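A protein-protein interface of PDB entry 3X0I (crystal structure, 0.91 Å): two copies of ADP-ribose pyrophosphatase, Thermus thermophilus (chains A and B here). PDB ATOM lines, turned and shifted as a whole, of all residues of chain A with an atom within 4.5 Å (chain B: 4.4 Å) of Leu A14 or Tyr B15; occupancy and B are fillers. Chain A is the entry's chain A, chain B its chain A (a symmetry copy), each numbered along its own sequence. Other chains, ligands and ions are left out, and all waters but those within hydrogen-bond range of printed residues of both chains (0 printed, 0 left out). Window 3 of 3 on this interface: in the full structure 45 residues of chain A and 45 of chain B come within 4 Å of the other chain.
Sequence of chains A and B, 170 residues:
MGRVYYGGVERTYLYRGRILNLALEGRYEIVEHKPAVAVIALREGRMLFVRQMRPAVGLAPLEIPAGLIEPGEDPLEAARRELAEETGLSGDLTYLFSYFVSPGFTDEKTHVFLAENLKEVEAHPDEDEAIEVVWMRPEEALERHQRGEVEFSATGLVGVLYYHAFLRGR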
ATOM      1  N   THR A  12      20.773  -0.657 -37.942  1.00  0.00           N
ATOM      2  CA  THR A  12      21.395  -1.611 -37.045  1.00  0.00           C
ATOM      3  C   THR A  12      21.582  -1.099 -35.625  1.00  0.00           C
ATOM      4  O   THR A  12      22.096  -0.024 -35.261  1.00  0.00           O
ATOM      5  CB  THR A  12      22.809  -1.898 -37.489  1.00  0.00           C
ATOM      6  OG1 THR A  12      22.664  -2.454 -38.806  1.00  0.00           O
ATOM      7  CG2 THR A  12      23.447  -2.969 -36.637  1.00  0.00           C
ATOM      8  N   TYR A  13      21.130  -1.929 -34.726  1.00  0.00           N
ATOM      9  CA  TYR A  13      21.107  -1.491 -33.348  1.00  0.00           C
ATOM     10  C   TYR A  13      22.407  -1.844 -32.650  1.00  0.00           C
ATOM     11  O   TYR A  13      22.812  -3.040 -32.637  1.00  0.00           O
ATOM     12  CB  TYR A  13      19.841  -2.088 -32.683  1.00  0.00           C
ATOM     13  CG  TYR A  13      18.643  -1.387 -33.294  1.00  0.00           C
ATOM     14  CD1 TYR A  13      18.008  -1.791 -34.437  1.00  0.00           C
ATOM     15  CD2 TYR A  13      18.183  -0.201 -32.672  1.00  0.00           C
ATOM     16  CE1 TYR A  13      16.941  -1.131 -34.998  1.00  0.00           C
ATOM     17  CE2 TYR A  13      17.082   0.503 -33.209  1.00  0.00           C
ATOM     18  CZ  TYR A  13      16.465   0.045 -34.357  1.00  0.00           C
ATOM     19  OH  TYR A  13      15.377   0.666 -34.950  1.00  0.00           O
ATOM     20  N   LEU A  14      23.048  -0.858 -32.047  1.00  0.00           N
ATOM     21  CA  LEU A  14      24.147  -1.071 -31.113  1.00  0.00           C
ATOM     22  C   LEU A  14      23.690  -1.220 -29.640  1.00  0.00           C
ATOM     23  O   LEU A  14      24.429  -1.882 -28.888  1.00  0.00           O
ATOM     24  CB  LEU A  14      25.149   0.063 -31.204  1.00  0.00           C
ATOM     25  CG  LEU A  14      25.613   0.430 -32.599  1.00  0.00           C
ATOM     26  CD1 LEU A  14      26.702   1.494 -32.513  1.00  0.00           C
ATOM     27  CD2 LEU A  14      26.172  -0.792 -33.311  1.00  0.00           C
ATOM     28  N   TYR A  15      22.557  -0.624 -29.279  1.00  0.00           N
ATOM     29  CA  TYR A  15      22.097  -0.670 -27.890  1.00  0.00           C
ATOM     30  C   TYR A  15      20.613  -0.428 -27.777  1.00  0.00           C
ATOM     31  O   TYR A  15      20.136   0.520 -28.426  1.00  0.00           O
ATOM     32  CB  TYR A  15      22.840   0.461 -27.126  1.00  0.00           C
ATOM     33  CG  TYR A  15      22.321   0.676 -25.726  1.00  0.00           C
ATOM     34  CD1 TYR A  15      22.664  -0.240 -24.722  1.00  0.00           C
ATOM     35  CD2 TYR A  15      21.491   1.688 -25.369  1.00  0.00           C
ATOM     36  CE1 TYR A  15      22.184  -0.085 -23.428  1.00  0.00           C
ATOM     37  CE2 TYR A  15      21.024   1.837 -24.075  1.00  0.00           C
ATOM     38  CZ  TYR A  15      21.363   0.969 -23.088  1.00  0.00           C
ATOM     39  OH  TYR A  15      20.934   1.088 -21.806  1.00  0.00           O
ATOM     40  N   LEU A  22      20.387   3.160 -29.456  1.00  0.00           N
ATOM     41  CA  LEU A  22      21.359   3.666 -30.333  1.00  0.00           C
ATOM     42  C   LEU A  22      21.441   2.764 -31.567  1.00  0.00           C
ATOM     43  O   LEU A  22      21.653   1.550 -31.521  1.00  0.00           O
ATOM     44  CB  LEU A  22      22.731   3.726 -29.653  1.00  0.00           C
ATOM     45  CG  LEU A  22      23.909   4.135 -30.504  1.00  0.00           C
ATOM     46  CD1 LEU A  22      23.778   5.576 -31.063  1.00  0.00           C
ATOM     47  CD2 LEU A  22      25.231   3.976 -29.758  1.00  0.00           C
ATOM     48  N   ALA A  23      21.341   3.375 -32.730  1.00  0.00           N
ATOM     49  CA  ALA A  23      21.343   2.662 -34.016  1.00  0.00           C
ATOM     50  C   ALA A  23      22.310   3.327 -34.966  1.00  0.00           C
ATOM     51  O   ALA A  23      22.589   4.555 -34.880  1.00  0.00           O
ATOM     52  CB  ALA A  23      19.959   2.540 -34.633  1.00  0.00           C
ATOM     53  N   LEU A  24      22.829   2.555 -35.895  1.00  0.00           N
ATOM     54  CA  LEU A  24      23.543   3.169 -37.021  1.00  0.00           C
ATOM     55  C   LEU A  24      22.667   2.977 -38.268  1.00  0.00           C
ATOM     56  O   LEU A  24      22.111   1.906 -38.504  1.00  0.00           O
ATOM     57  CB  LEU A  24      24.907   2.587 -37.364  1.00  0.00           C
ATOM     58  CG  LEU A  24      25.837   2.545 -36.135  1.00  0.00           C
ATOM     59  CD1 LEU A  24      27.047   1.655 -36.448  1.00  0.00           C
ATOM     60  CD2 LEU A  24      26.083   3.990 -35.794  1.00  0.00           C
ATOM     61  N   GLU A  29      24.623   8.113 -36.993  1.00  0.00           N
ATOM     62  CA  GLU A  29      24.417   7.689 -35.621  1.00  0.00           C
ATOM     63  C   GLU A  29      23.065   8.238 -35.158  1.00  0.00           C
ATOM     64  O   GLU A  29      22.832   9.445 -35.196  1.00  0.00           O
ATOM     65  CB  GLU A  29      25.535   8.195 -34.710  1.00  0.00           C
ATOM     66  CG  GLU A  29      26.907   7.686 -35.156  1.00  0.00           C
ATOM     67  CD  GLU A  29      28.048   8.571 -34.664  1.00  0.00           C
ATOM     68  OE1 GLU A  29      28.011   9.801 -34.666  1.00  0.00           O
ATOM     69  OE2 GLU A  29      29.007   7.912 -34.196  1.00  0.00           O
ATOM     70  N   TYR B  13      31.545   3.983 -20.723  1.00  0.00           N
ATOM     71  CA  TYR B  13      31.217   4.198 -22.115  1.00  0.00           C
ATOM     72  C   TYR B  13      30.810   2.895 -22.778  1.00  0.00           C
ATOM     73  O   TYR B  13      31.585   1.899 -22.744  1.00  0.00           O
ATOM     74  CB  TYR B  13      32.424   4.904 -22.783  1.00  0.00           C
ATOM     75  CG  TYR B  13      32.487   6.310 -22.217  1.00  0.00           C
ATOM     76  CD1 TYR B  13      33.152   6.656 -21.072  1.00  0.00           C
ATOM     77  CD2 TYR B  13      31.761   7.326 -22.885  1.00  0.00           C
ATOM     78  CE1 TYR B  13      33.179   7.928 -20.552  1.00  0.00           C
ATOM     79  CE2 TYR B  13      31.768   8.649 -22.392  1.00  0.00           C
ATOM     80  CZ  TYR B  13      32.470   8.951 -21.241  1.00  0.00           C
ATOM     81  OH  TYR B  13      32.540  10.220 -20.688  1.00  0.00           O
ATOM     82  N   LEU B  14      29.644   2.882 -23.402  1.00  0.00           N
ATOM     83  CA  LEU B  14      29.234   1.816 -24.308  1.00  0.00           C
ATOM     84  C   LEU B  14      29.636   2.067 -25.784  1.00  0.00           C
ATOM     85  O   LEU B  14      29.796   1.062 -26.500  1.00  0.00           O
ATOM     86  CB  LEU B  14      27.735   1.605 -24.237  1.00  0.00           C
ATOM     87  CG  LEU B  14      27.147   1.466 -22.846  1.00  0.00           C
ATOM     88  CD1 LEU B  14      25.662   1.138 -22.949  1.00  0.00           C
ATOM     89  CD2 LEU B  14      27.848   0.351 -22.085  1.00  0.00           C
ATOM     90  N   TYR B  15      29.769   3.328 -26.184  1.00  0.00           N
ATOM     91  CA  TYR B  15      30.084   3.641 -27.579  1.00  0.00           C
ATOM     92  C   TYR B  15      30.701   5.010 -27.726  1.00  0.00           C
ATOM     93  O   TYR B  15      30.161   5.950 -27.118  1.00  0.00           O
ATOM     94  CB  TYR B  15      28.745   3.616 -28.367  1.00  0.00           C
ATOM     95  CG  TYR B  15      28.877   4.122 -29.782  1.00  0.00           C
ATOM     96  CD1 TYR B  15      29.471   3.298 -30.749  1.00  0.00           C
ATOM     97  CD2 TYR B  15      28.494   5.359 -30.187  1.00  0.00           C
ATOM     98  CE1 TYR B  15      29.628   3.741 -32.056  1.00  0.00           C
ATOM     99  CE2 TYR B  15      28.650   5.787 -31.493  1.00  0.00           C
ATOM    100  CZ  TYR B  15      29.206   4.996 -32.445  1.00  0.00           C
ATOM    101  OH  TYR B  15      29.366   5.375 -33.737  1.00  0.00           O
ATOM    102  N   ARG B  16      31.718   5.108 -28.537  1.00  0.00           N
ATOM    103  CA  ARG B  16      32.395   6.347 -28.776  1.00  0.00           C
ATOM    104  C   ARG B  16      32.328   6.556 -30.279  1.00  0.00           C
ATOM    105  O   ARG B  16      32.894   5.774 -31.001  1.00  0.00           O
ATOM    106  CB  ARG B  16      33.814   6.342 -28.266  1.00  0.00           C
ATOM    107  CG  ARG B  16      33.950   6.337 -26.754  1.00  0.00           C
ATOM    108  CD  ARG B  16      35.435   6.365 -26.421  1.00  0.00           C
ATOM    109  NE  ARG B  16      35.718   6.535 -25.013  1.00  0.00           N
ATOM    110  CZ  ARG B  16      35.691   7.636 -24.276  1.00  0.00           C
ATOM    111  NH1 ARG B  16      35.372   8.844 -24.757  1.00  0.00           N
ATOM    112  NH2 ARG B  16      36.003   7.523 -22.970  1.00  0.00           N
ATOM    113  N   GLY B  17      31.597   7.614 -30.701  1.00  0.00           N
ATOM    114  CA  GLY B  17      31.330   7.848 -32.096  1.00  0.00           C
ATOM    115  C   GLY B  17      31.817   9.169 -32.620  1.00  0.00           C
ATOM    116  O   GLY B  17      32.723   9.739 -32.018  1.00  0.00           O
ATOM    117  N   LEU B  20      28.685  11.677 -31.226  1.00  0.00           N
ATOM    118  CA  LEU B  20      28.126  11.347 -29.930  1.00  0.00           C
ATOM    119  C   LEU B  20      28.882  10.185 -29.311  1.00  0.00           C
ATOM    120  O   LEU B  20      29.462   9.403 -30.047  1.00  0.00           O
ATOM    121  CB  LEU B  20      26.616  11.014 -30.030  1.00  0.00           C
ATOM    122  CG  LEU B  20      26.175   9.719 -30.793  1.00  0.00           C
ATOM    123  CD1 LEU B  20      26.199   8.477 -29.971  1.00  0.00           C
ATOM    124  CD2 LEU B  20      24.728   9.980 -31.317  1.00  0.00           C
ATOM    125  N   ASN B  21      28.778  10.126 -27.998  1.00  0.00           N
ATOM    126  CA  ASN B  21      29.161   8.969 -27.211  1.00  0.00           C
ATOM    127  C   ASN B  21      27.915   8.545 -26.425  1.00  0.00           C
ATOM    128  O   ASN B  21      27.144   9.372 -26.028  1.00  0.00           O
ATOM    129  CB  ASN B  21      30.268   9.252 -26.194  1.00  0.00           C
ATOM    130  CG  ASN B  21      31.510   9.850 -26.873  1.00  0.00           C
ATOM    131  OD1 ASN B  21      31.899   9.412 -27.944  1.00  0.00           O
ATOM    132  ND2 ASN B  21      32.012  10.830 -26.206  1.00  0.00           N
ATOM    133  N   LEU B  22      27.800   7.224 -26.172  1.00  0.00           N
ATOM    134  CA  LEU B  22      26.827   6.720 -25.295  1.00  0.00           C
ATOM    135  C   LEU B  22      27.513   6.197 -24.030  1.00  0.00           C
ATOM    136  O   LEU B  22      28.411   5.352 -24.032  1.00  0.00           O
ATOM    137  CB  LEU B  22      26.035   5.586 -25.951  1.00  0.00           C
ATOM    138  CG  LEU B  22      25.029   4.854 -25.094  1.00  0.00           C
ATOM    139  CD1 LEU B  22      23.889   5.774 -24.586  1.00  0.00           C
ATOM    140  CD2 LEU B  22      24.448   3.639 -25.810  1.00  0.00           C
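OE2 of Glu A29 lies within hydrogen-bond range of OH of Tyr B15, at 2.6 Å.
O of Leu A22 is in hydrogen-bond range of N of Leu A14.
The backbone carbonyl oxygen (O) of Leu B22 is in hydrogen-bond range of the backbone NH (N) of Leu B14, at 2.8 Å.
N of Leu A22 sits at hydrogen-bond distance from O of Tyr A15 (2.8 Å).
The backbone NH (N) of Gly B17 is in hydrogen-bond range of the side-chain amide oxygen (OD1) of Asn B21 (3.3 Å).
The backbone carbonyl oxygen (O) of Tyr B15 lies within hydrogen-bond range of the backbone NH (N) of Leu B22.
Among the printed residues, merely in contact across the chains: Leu A14 with Tyr B15, Tyr A15 with Leu B14, Tyr A15 with Leu B22, Leu A22 with Tyr B15, Leu A22 with Leu B20, Glu A29 with Gly B17 and Glu A29 with Leu B20.
Printed residues of chain A within 4 Å of Tyr B15: Leu A14 (3.7 Å), Leu A22 (3.6 Å) and Glu A29 (2.6 Å).
Of the printed residues of chain A, Leu B20 touches Leu A22 and Glu A29.
Printed residues of chain B within 4 Å of Leu A22: Tyr B15 and Leu B20.
Printed residues of chain B within 4 Å of Tyr A15: Leu B14 (3.7 Å) and Leu B22 (3.6 Å).
Tyr A13 touches none of the printed residues of chain B.
Ala A23 touches none of the printed residues of chain B.
The nearest residue of chain A that does not touch Tyr B15 is Leu A24 (4.1 Å).
Of the 8 printed residues of chain B, 5 touch a printed residue of chain A.
Hydrophobic or aromatic side chains of chain B within 4 Å of the printed part of chain A: Leu B14, Tyr B15, Leu B20 and Leu B22.
Of the 8 printed residues of chain A, 4 touch a printed residue of chain B.
Hydrophobic or aromatic side chains of chain A within 4 Å of the printed part of chain B: Leu A14, Tyr A15 and Leu A22.
Among the printed residues, no Asp or Glu carboxylate lies within 4 Å of a Lys or Arg side-chain nitrogen of the other chain.
Leu A14 touches Tyr B15, and with the chains exchanged Tyr A15 touches Leu B14.
Tyr A15 touches Leu B22, and with the chains exchanged Leu A22 touches Tyr B15.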
